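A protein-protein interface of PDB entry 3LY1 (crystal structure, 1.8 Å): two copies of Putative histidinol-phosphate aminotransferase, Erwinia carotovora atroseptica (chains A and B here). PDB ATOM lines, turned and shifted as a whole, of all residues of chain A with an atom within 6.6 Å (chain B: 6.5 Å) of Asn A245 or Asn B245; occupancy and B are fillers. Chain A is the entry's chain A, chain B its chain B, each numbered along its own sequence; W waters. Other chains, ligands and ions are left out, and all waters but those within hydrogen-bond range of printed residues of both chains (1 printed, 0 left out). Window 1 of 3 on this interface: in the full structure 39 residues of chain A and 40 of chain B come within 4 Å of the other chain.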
ATOM      1  N   ALA A  49      14.919   5.832 -24.560  1.00  0.00           N
ATOM      2  CA  ALA A  49      14.933   6.408 -25.898  1.00  0.00           C
ATOM      3  C   ALA A  49      16.138   5.934 -26.710  1.00  0.00           C
ATOM      4  O   ALA A  49      16.798   6.755 -27.367  1.00  0.00           O
ATOM      5  CB  ALA A  49      14.924   7.959 -25.822  1.00  0.00           C
ATOM      6  N   ILE A  53      18.038   8.238 -29.575  1.00  0.00           N
ATOM      7  CA  ILE A  53      19.375   8.751 -29.210  1.00  0.00           C
ATOM      8  C   ILE A  53      20.389   8.484 -30.322  1.00  0.00           C
ATOM      9  O   ILE A  53      21.219   9.338 -30.635  1.00  0.00           O
ATOM     10  CB  ILE A  53      19.816   8.193 -27.885  1.00  0.00           C
ATOM     11  CG1 ILE A  53      19.040   8.919 -26.769  1.00  0.00           C
ATOM     12  CG2 ILE A  53      21.383   8.279 -27.684  1.00  0.00           C
ATOM     13  CD1 ILE A  53      19.094   8.223 -25.375  1.00  0.00           C
ATOM     14  N   ALA A 218      16.867  24.742 -21.875  1.00  0.00           N
ATOM     15  CA  ALA A 218      17.687  24.586 -20.674  1.00  0.00           C
ATOM     16  C   ALA A 218      17.155  23.444 -19.805  1.00  0.00           C
ATOM     17  O   ALA A 218      17.904  22.607 -19.427  1.00  0.00           O
ATOM     18  CB  ALA A 218      17.776  25.911 -19.852  1.00  0.00           C
ATOM     19  N   GLY A 219      15.851  23.395 -19.550  1.00  0.00           N
ATOM     20  CA  GLY A 219      15.313  22.389 -18.631  1.00  0.00           C
ATOM     21  C   GLY A 219      15.169  21.002 -19.223  1.00  0.00           C
ATOM     22  O   GLY A 219      14.747  20.097 -18.537  1.00  0.00           O
ATOM     23  N   MET A 220      15.478  20.845 -20.496  1.00  0.00           N
ATOM     24  CA  MET A 220      15.401  19.560 -21.164  1.00  0.00           C
ATOM     25  C   MET A 220      16.719  18.770 -21.107  1.00  0.00           C
ATOM     26  O   MET A 220      16.724  17.560 -21.346  1.00  0.00           O
ATOM     27  CB  MET A 220      14.937  19.742 -22.593  1.00  0.00           C
ATOM     28  CG  MET A 220      13.539  20.223 -22.721  1.00  0.00           C
ATOM     29  SD  MET A 220      12.192  18.746 -22.599  1.00  0.00           S
ATOM     30  CE  MET A 220      11.863  18.827 -20.656  1.00  0.00           C
ATOM     31  N   ARG A 221      17.814  19.426 -20.702  1.00  0.00           N
ATOM     32  CA  ARG A 221      19.093  18.765 -20.477  1.00  0.00           C
ATOM     33  C   ARG A 221      19.610  17.967 -21.697  1.00  0.00           C
ATOM     34  O   ARG A 221      19.741  16.738 -21.652  1.00  0.00           O
ATOM     35  CB  ARG A 221      19.061  17.905 -19.189  1.00  0.00           C
ATOM     36  CG  ARG A 221      18.282  18.545 -18.025  1.00  0.00           C
ATOM     37  CD  ARG A 221      18.802  19.931 -17.639  1.00  0.00           C
ATOM     38  NE  ARG A 221      20.257  19.938 -17.362  1.00  0.00           N
ATOM     39  CZ  ARG A 221      21.139  20.753 -17.935  1.00  0.00           C
ATOM     40  NH1 ARG A 221      20.734  21.674 -18.791  1.00  0.00           N
ATOM     41  NH2 ARG A 221      22.432  20.672 -17.624  1.00  0.00           N
ATOM     42  N   VAL A 222      19.909  18.683 -22.775  1.00  0.00           N
ATOM     43  CA  VAL A 222      20.505  18.086 -23.953  1.00  0.00           C
ATOM     44  C   VAL A 222      21.678  18.930 -24.402  1.00  0.00           C
ATOM     45  O   VAL A 222      21.520  20.088 -24.741  1.00  0.00           O
ATOM     46  CB  VAL A 222      19.480  17.924 -25.135  1.00  0.00           C
ATOM     47  CG1 VAL A 222      20.093  17.067 -26.258  1.00  0.00           C
ATOM     48  CG2 VAL A 222      18.116  17.336 -24.666  1.00  0.00           C
ATOM     49  N   LYS A 243      22.225   8.451 -22.452  1.00  0.00           N
ATOM     50  CA  LYS A 243      20.902   8.045 -21.991  1.00  0.00           C
ATOM     51  C   LYS A 243      20.108   9.320 -21.682  1.00  0.00           C
ATOM     52  O   LYS A 243      19.702   9.568 -20.537  1.00  0.00           O
ATOM     53  CB  LYS A 243      21.017   7.154 -20.751  1.00  0.00           C
ATOM     54  CG  LYS A 243      21.847   5.884 -20.968  1.00  0.00           C
ATOM     55  CD  LYS A 243      21.907   5.043 -19.740  1.00  0.00           C
ATOM     56  CE  LYS A 243      22.679   3.742 -19.983  1.00  0.00           C
ATOM     57  NZ  LYS A 243      22.626   2.844 -18.824  1.00  0.00           N
ATOM     58  N   ILE A 244      19.917  10.104 -22.727  1.00  0.00           N
ATOM     59  CA  ILE A 244      19.239  11.391 -22.675  1.00  0.00           C
ATOM     60  C   ILE A 244      17.754  11.113 -22.507  1.00  0.00           C
ATOM     61  O   ILE A 244      17.242  10.086 -22.945  1.00  0.00           O
ATOM     62  CB  ILE A 244      19.562  12.214 -23.975  1.00  0.00           C
ATOM     63  CG1 ILE A 244      21.083  12.343 -24.153  1.00  0.00           C
ATOM     64  CG2 ILE A 244      19.040  13.621 -23.902  1.00  0.00           C
ATOM     65  CD1 ILE A 244      21.780  12.994 -22.938  1.00  0.00           C
ATOM     66  N   ASN A 245      17.050  12.039 -21.880  1.00  0.00           N
ATOM     67  CA  ASN A 245      15.640  11.866 -21.624  1.00  0.00           C
ATOM     68  C   ASN A 245      14.809  11.958 -22.914  1.00  0.00           C
ATOM     69  O   ASN A 245      15.193  12.647 -23.869  1.00  0.00           O
ATOM     70  CB  ASN A 245      15.163  12.812 -20.519  1.00  0.00           C
ATOM     71  CG  ASN A 245      14.746  14.151 -21.023  1.00  0.00           C
ATOM     72  OD1 ASN A 245      13.610  14.347 -21.473  1.00  0.00           O
ATOM     73  ND2 ASN A 245      15.653  15.097 -20.942  1.00  0.00           N
ATOM     74  N   PHE A 246      13.723  11.196 -22.956  1.00  0.00           N
ATOM     75  CA  PHE A 246      12.911  11.038 -24.174  1.00  0.00           C
ATOM     76  C   PHE A 246      12.345  12.358 -24.699  1.00  0.00           C
ATOM     77  O   PHE A 246      12.408  12.624 -25.877  1.00  0.00           O
ATOM     78  CB  PHE A 246      11.754  10.062 -23.928  1.00  0.00           C
ATOM     79  CG  PHE A 246      11.541   9.084 -25.031  1.00  0.00           C
ATOM     80  CD1 PHE A 246      11.378   9.508 -26.351  1.00  0.00           C
ATOM     81  CD2 PHE A 246      11.399   7.739 -24.749  1.00  0.00           C
ATOM     82  CE1 PHE A 246      11.149   8.598 -27.344  1.00  0.00           C
ATOM     83  CE2 PHE A 246      11.156   6.820 -25.752  1.00  0.00           C
ATOM     84  CZ  PHE A 246      11.047   7.245 -27.045  1.00  0.00           C
ATOM     85  N   SER A 247      11.806  13.195 -23.828  1.00  0.00           N
ATOM     86  CA  SER A 247      11.233  14.458 -24.295  1.00  0.00           C
ATOM     87  C   SER A 247      12.329  15.359 -24.855  1.00  0.00           C
ATOM     88  O   SER A 247      12.137  15.980 -25.876  1.00  0.00           O
ATOM     89  CB  SER A 247      10.480  15.189 -23.172  1.00  0.00           C
ATOM     90  OG  SER A 247       9.413  14.386 -22.719  1.00  0.00           O
ATOM     91  N   GLY A 248      13.466  15.418 -24.178  1.00  0.00           N
ATOM     92  CA  GLY A 248      14.588  16.178 -24.658  1.00  0.00           C
ATOM     93  C   GLY A 248      15.132  15.717 -25.999  1.00  0.00           C
ATOM     94  O   GLY A 248      15.411  16.558 -26.858  1.00  0.00           O
ATOM     95  N   VAL A 249      15.261  14.398 -26.183  1.00  0.00           N
ATOM     96  CA  VAL A 249      15.780  13.839 -27.433  1.00  0.00           C
ATOM     97  C   VAL A 249      14.819  14.183 -28.592  1.00  0.00           C
ATOM     98  O   VAL A 249      15.237  14.659 -29.647  1.00  0.00           O
ATOM     99  CB  VAL A 249      15.976  12.313 -27.362  1.00  0.00           C
ATOM    100  CG1 VAL A 249      16.231  11.749 -28.739  1.00  0.00           C
ATOM    101  CG2 VAL A 249      17.120  11.962 -26.386  1.00  0.00           C
ATOM    102  N   ASP A 250      13.529  13.960 -28.390  1.00  0.00           N
ATOM    103  CA  ASP A 250      12.547  14.259 -29.442  1.00  0.00           C
ATOM    104  C   ASP A 250      12.386  15.781 -29.641  1.00  0.00           C
ATOM    105  O   ASP A 250      12.126  16.246 -30.764  1.00  0.00           O
ATOM    106  CB  ASP A 250      11.187  13.629 -29.123  1.00  0.00           C
ATOM    107  CG  ASP A 250      11.107  12.123 -29.457  1.00  0.00           C
ATOM    108  OD1 ASP A 250      12.094  11.529 -29.962  1.00  0.00           O
ATOM    109  OD2 ASP A 250      10.012  11.543 -29.253  1.00  0.00           O
ATOM    110  N   ALA B  49      14.988  23.748 -13.898  1.00  0.00           N
ATOM    111  CA  ALA B  49      14.088  23.348 -12.788  1.00  0.00           C
ATOM    112  C   ALA B  49      14.723  23.502 -11.392  1.00  0.00           C
ATOM    113  O   ALA B  49      14.675  22.563 -10.572  1.00  0.00           O
ATOM    114  CB  ALA B  49      13.696  21.901 -12.994  1.00  0.00           C
ATOM    115  N   ILE B  53      13.841  20.900  -8.291  1.00  0.00           N
ATOM    116  CA  ILE B  53      14.887  19.948  -7.862  1.00  0.00           C
ATOM    117  C   ILE B  53      15.087  19.997  -6.355  1.00  0.00           C
ATOM    118  O   ILE B  53      15.235  18.950  -5.700  1.00  0.00           O
ATOM    119  CB  ILE B  53      16.199  20.210  -8.647  1.00  0.00           C
ATOM    120  CG1 ILE B  53      16.027  19.714 -10.086  1.00  0.00           C
ATOM    121  CG2 ILE B  53      17.459  19.546  -8.004  1.00  0.00           C
ATOM    122  CD1 ILE B  53      16.979  20.338 -11.094  1.00  0.00           C
ATOM    123  N   ALA B 218      11.397   5.205 -17.237  1.00  0.00           N
ATOM    124  CA  ALA B 218      12.779   4.962 -17.669  1.00  0.00           C
ATOM    125  C   ALA B 218      13.331   6.072 -18.569  1.00  0.00           C
ATOM    126  O   ALA B 218      14.478   6.477 -18.403  1.00  0.00           O
ATOM    127  CB  ALA B 218      12.949   3.572 -18.367  1.00  0.00           C
ATOM    128  N   GLY B 219      12.534   6.520 -19.528  1.00  0.00           N
ATOM    129  CA  GLY B 219      12.943   7.568 -20.447  1.00  0.00           C
ATOM    130  C   GLY B 219      13.022   8.978 -19.857  1.00  0.00           C
ATOM    131  O   GLY B 219      13.501   9.893 -20.502  1.00  0.00           O
ATOM    132  N   MET B 220      12.541   9.154 -18.639  1.00  0.00           N
ATOM    133  CA  MET B 220      12.509  10.461 -17.998  1.00  0.00           C
ATOM    134  C   MET B 220      13.828  10.749 -17.261  1.00  0.00           C
ATOM    135  O   MET B 220      14.140  11.920 -17.006  1.00  0.00           O
ATOM    136  CB  MET B 220      11.356  10.565 -17.027  1.00  0.00           C
ATOM    137  CG  MET B 220       9.943  10.741 -17.672  1.00  0.00           C
ATOM    138  SD  MET B 220       9.694  12.492 -18.450  1.00  0.00           S
ATOM    139  CE  MET B 220      10.291  12.148 -20.276  1.00  0.00           C
ATOM    140  N   ARG B 221      14.590   9.716 -16.938  1.00  0.00           N
ATOM    141  CA  ARG B 221      15.954   9.835 -16.351  1.00  0.00           C
ATOM    142  C   ARG B 221      16.031  10.498 -14.945  1.00  0.00           C
ATOM    143  O   ARG B 221      16.700  11.541 -14.749  1.00  0.00           O
ATOM    144  CB  ARG B 221      16.958  10.510 -17.333  1.00  0.00           C
ATOM    145  CG  ARG B 221      16.831  10.085 -18.820  1.00  0.00           C
ATOM    146  CD  ARG B 221      16.920   8.538 -19.016  1.00  0.00           C
ATOM    147  NE  ARG B 221      18.155   7.981 -18.447  1.00  0.00           N
ATOM    148  CZ  ARG B 221      18.230   6.967 -17.591  1.00  0.00           C
ATOM    149  NH1 ARG B 221      17.140   6.312 -17.175  1.00  0.00           N
ATOM    150  NH2 ARG B 221      19.417   6.582 -17.154  1.00  0.00           N
ATOM    151  N   VAL B 222      15.397   9.865 -13.956  1.00  0.00           N
ATOM    152  CA  VAL B 222      15.380  10.371 -12.599  1.00  0.00           C
ATOM    153  C   VAL B 222      15.708   9.209 -11.701  1.00  0.00           C
ATOM    154  O   VAL B 222      14.993   8.201 -11.673  1.00  0.00           O
ATOM    155  CB  VAL B 222      14.014  10.955 -12.214  1.00  0.00           C
ATOM    156  CG1 VAL B 222      14.101  11.642 -10.883  1.00  0.00           C
ATOM    157  CG2 VAL B 222      13.452  11.895 -13.340  1.00  0.00           C
ATOM    158  N   LYS B 243      20.876  18.505 -11.865  1.00  0.00           N
ATOM    159  CA  LYS B 243      20.281  19.280 -12.962  1.00  0.00           C
ATOM    160  C   LYS B 243      19.397  18.386 -13.809  1.00  0.00           C
ATOM    161  O   LYS B 243      19.528  18.294 -15.039  1.00  0.00           O
ATOM    162  CB  LYS B 243      21.345  19.988 -13.829  1.00  0.00           C
ATOM    163  CG  LYS B 243      22.327  20.831 -13.047  1.00  0.00           C
ATOM    164  CD  LYS B 243      23.255  21.686 -13.980  1.00  0.00           C
ATOM    165  CE  LYS B 243      24.254  22.504 -13.145  1.00  0.00           C
ATOM    166  NZ  LYS B 243      25.321  23.211 -13.935  1.00  0.00           N
ATOM    167  N   ILE B 244      18.440  17.786 -13.132  1.00  0.00           N
ATOM    168  CA  ILE B 244      17.516  16.835 -13.711  1.00  0.00           C
ATOM    169  C   ILE B 244      16.559  17.598 -14.604  1.00  0.00           C
ATOM    170  O   ILE B 244      16.280  18.767 -14.364  1.00  0.00           O
ATOM    171  CB  ILE B 244      16.719  16.159 -12.555  1.00  0.00           C
ATOM    172  CG1 ILE B 244      17.693  15.571 -11.545  1.00  0.00           C
ATOM    173  CG2 ILE B 244      15.821  15.077 -13.048  1.00  0.00           C
ATOM    174  CD1 ILE B 244      18.777  14.672 -12.215  1.00  0.00           C
ATOM    175  N   ASN B 245      16.037  16.924 -15.618  1.00  0.00           N
ATOM    176  CA  ASN B 245      15.167  17.587 -16.591  1.00  0.00           C
ATOM    177  C   ASN B 245      13.807  17.933 -16.007  1.00  0.00           C
ATOM    178  O   ASN B 245      13.301  17.216 -15.133  1.00  0.00           O
ATOM    179  CB  ASN B 245      15.072  16.792 -17.884  1.00  0.00           C
ATOM    180  CG  ASN B 245      14.045  15.701 -17.845  1.00  0.00           C
ATOM    181  OD1 ASN B 245      12.856  15.927 -18.153  1.00  0.00           O
ATOM    182  ND2 ASN B 245      14.486  14.494 -17.488  1.00  0.00           N
ATOM    183  N   PHE B 246      13.240  19.043 -16.475  1.00  0.00           N
ATOM    184  CA  PHE B 246      11.977  19.567 -15.917  1.00  0.00           C
ATOM    185  C   PHE B 246      10.810  18.582 -15.949  1.00  0.00           C
ATOM    186  O   PHE B 246      10.103  18.443 -14.940  1.00  0.00           O
ATOM    187  CB  PHE B 246      11.514  20.843 -16.625  1.00  0.00           C
ATOM    188  CG  PHE B 246      11.080  21.960 -15.670  1.00  0.00           C
ATOM    189  CD1 PHE B 246      10.198  21.724 -14.631  1.00  0.00           C
ATOM    190  CD2 PHE B 246      11.557  23.238 -15.834  1.00  0.00           C
ATOM    191  CE1 PHE B 246       9.811  22.757 -13.776  1.00  0.00           C
ATOM    192  CE2 PHE B 246      11.167  24.271 -14.992  1.00  0.00           C
ATOM    193  CZ  PHE B 246      10.299  24.028 -13.961  1.00  0.00           C
ATOM    194  N   SER B 247      10.596  17.899 -17.073  1.00  0.00           N
ATOM    195  CA  SER B 247       9.530  16.917 -17.131  1.00  0.00           C
ATOM    196  C   SER B 247       9.681  15.768 -16.146  1.00  0.00           C
ATOM    197  O   SER B 247       8.688  15.333 -15.560  1.00  0.00           O
ATOM    198  CB  SER B 247       9.322  16.393 -18.558  1.00  0.00           C
ATOM    199  OG  SER B 247       8.931  17.461 -19.413  1.00  0.00           O
ATOM    200  N   GLY B 248      10.917  15.296 -15.946  1.00  0.00           N
ATOM    201  CA  GLY B 248      11.193  14.184 -15.056  1.00  0.00           C
ATOM    202  C   GLY B 248      11.004  14.598 -13.605  1.00  0.00           C
ATOM    203  O   GLY B 248      10.453  13.838 -12.812  1.00  0.00           O
ATOM    204  N   VAL B 249      11.436  15.816 -13.269  1.00  0.00           N
ATOM    205  CA  VAL B 249      11.299  16.346 -11.918  1.00  0.00           C
ATOM    206  C   VAL B 249       9.845  16.446 -11.512  1.00  0.00           C
ATOM    207  O   VAL B 249       9.477  15.977 -10.417  1.00  0.00           O
ATOM    208  CB  VAL B 249      12.030  17.706 -11.728  1.00  0.00           C
ATOM    209  CG1 VAL B 249      11.772  18.260 -10.365  1.00  0.00           C
ATOM    210  CG2 VAL B 249      13.524  17.505 -11.906  1.00  0.00           C
ATOM    211  N   ASP B 250       9.029  17.038 -12.383  1.00  0.00           N
ATOM    212  CA  ASP B 250       7.620  17.229 -12.094  1.00  0.00           C
ATOM    213  C   ASP B 250       6.859  15.900 -12.120  1.00  0.00           C
ATOM    214  O   ASP B 250       5.974  15.689 -11.301  1.00  0.00           O
ATOM    215  CB  ASP B 250       6.985  18.244 -13.062  1.00  0.00           C
ATOM    216  CG  ASP B 250       7.254  19.701 -12.668  1.00  0.00           C
ATOM    217  OD1 ASP B 250       8.042  19.932 -11.713  1.00  0.00           O
ATOM    218  OD2 ASP B 250       6.696  20.616 -13.302  1.00  0.00           O
HETATM  219  O   HOH W   1      21.247   8.834 -17.699  1.00  0.00           O
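Of the printed residues of chain B, Met A220 touches Asn B245 (3.9 Å) and Ser B247 (3.5 Å).
Printed residues of chain B within 4 Å of Arg A221: Lys B243 (2.9 Å), Ile B244 (3.9 Å) and Asn B245 (3.6 Å).
Of the printed residues of chain B, Lys A243 touches Arg B221.
Asn A245 touches just these residues of chain B: Gly B219 (3.1 Å), Met B220 (3.8 Å), Arg B221 (3.5 Å) and Asn B245 (3.5 Å).
Gly A248 touches none of the printed residues of chain B.
Of chain A, only Gly A219, Met A220, Arg A221 and Asn A245 come within 4 Å of Asn B245.
Of the printed residues of chain A, Phe B246 touches Gly A219.
The nearest residue of chain A that does not touch Asn B245 is Ser A247 (5.6 Å).
O of Ala A218 is in hydrogen-bond range of NH1 of Arg A221 (3.0 Å).
OD1 of Asn A245 sits at hydrogen-bond distance from N of Ser A247, at 3.2 Å.
The side-chain amide oxygen (OD1) of Asn A245 is in hydrogen-bond range of the backbone NH (N) of Gly A248 (2.9 Å).
O of Met B220 lies within hydrogen-bond range of ND2 of Asn B245, at 2.6 Å.
OD1 of Asn B245 lies within hydrogen-bond range of N of Ser B247 (3.2 Å).
OD1 of Asn B245 is in hydrogen-bond range of N of Gly B248 (3.0 Å).
Gly A219 touches Asn B245, and with the chains exchanged Asn A245 touches Gly B219.
Gly A219 touches Phe B246, and with the chains exchanged Phe A246 touches Gly B219.
Arg A221 touches Lys B243, and with the chains exchanged Lys A243 touches Arg B221.
Arg A221 touches Asn B245, and with the chains exchanged Asn A245 touches Arg B221.
The backbone carbonyl oxygen of Gly A219 is in hydrogen-bond range of the backbone NH of Phe B246 (2.8 Å).
The guanidinium group (NE) of Arg A221 lies within hydrogen-bond range of the backbone carbonyl oxygen (O) of Lys B243.
The backbone carbonyl oxygen (O) of Lys A243 is in hydrogen-bond range of the guanidinium group (NE) of Arg B221 (3.0 Å).
The backbone NH (N) of Phe A246 sits at hydrogen-bond distance from the backbone carbonyl oxygen (O) of Gly B219 (2.8 Å).
Among the printed residues, pairs that only touch across the chains: Gly A219 with Asn B245 (3.2 Å), Met A220 with Asn B245 (3.9 Å), Met A220 with Ser B247 (3.5 Å), Arg A221 with Ile B244 (3.9 Å), Arg A221 with Asn B245 (3.6 Å), Ile A244 with Arg B221 (3.9 Å), Asn A245 with Gly B219 (3.1 Å), Asn A245 with Met B220 (3.8 Å), Asn A245 with Arg B221 (3.5 Å), Asn A245 with Asn B245 (3.5 Å) and Ser A247 with Met B220 (3.4 Å).
Water W1 lies within hydrogen-bond range of the guanidinium group of Arg B221 (3.0 Å) and the backbone carbonyl oxygen of Lys A243 (3.3 Å).
Printed residues of chain B that touch a printed residue of chain A: Gly B219, Met B220, Arg B221, Lys B243, Ile B244, Asn B245, Phe B246 and Ser B247.
Of the 15 printed residues of chain A, 8 touch a printed residue of chain B.
Among the printed residues, no Asp or Glu carboxylate lies within 4 Å of a Lys or Arg side-chain nitrogen of the other chain.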
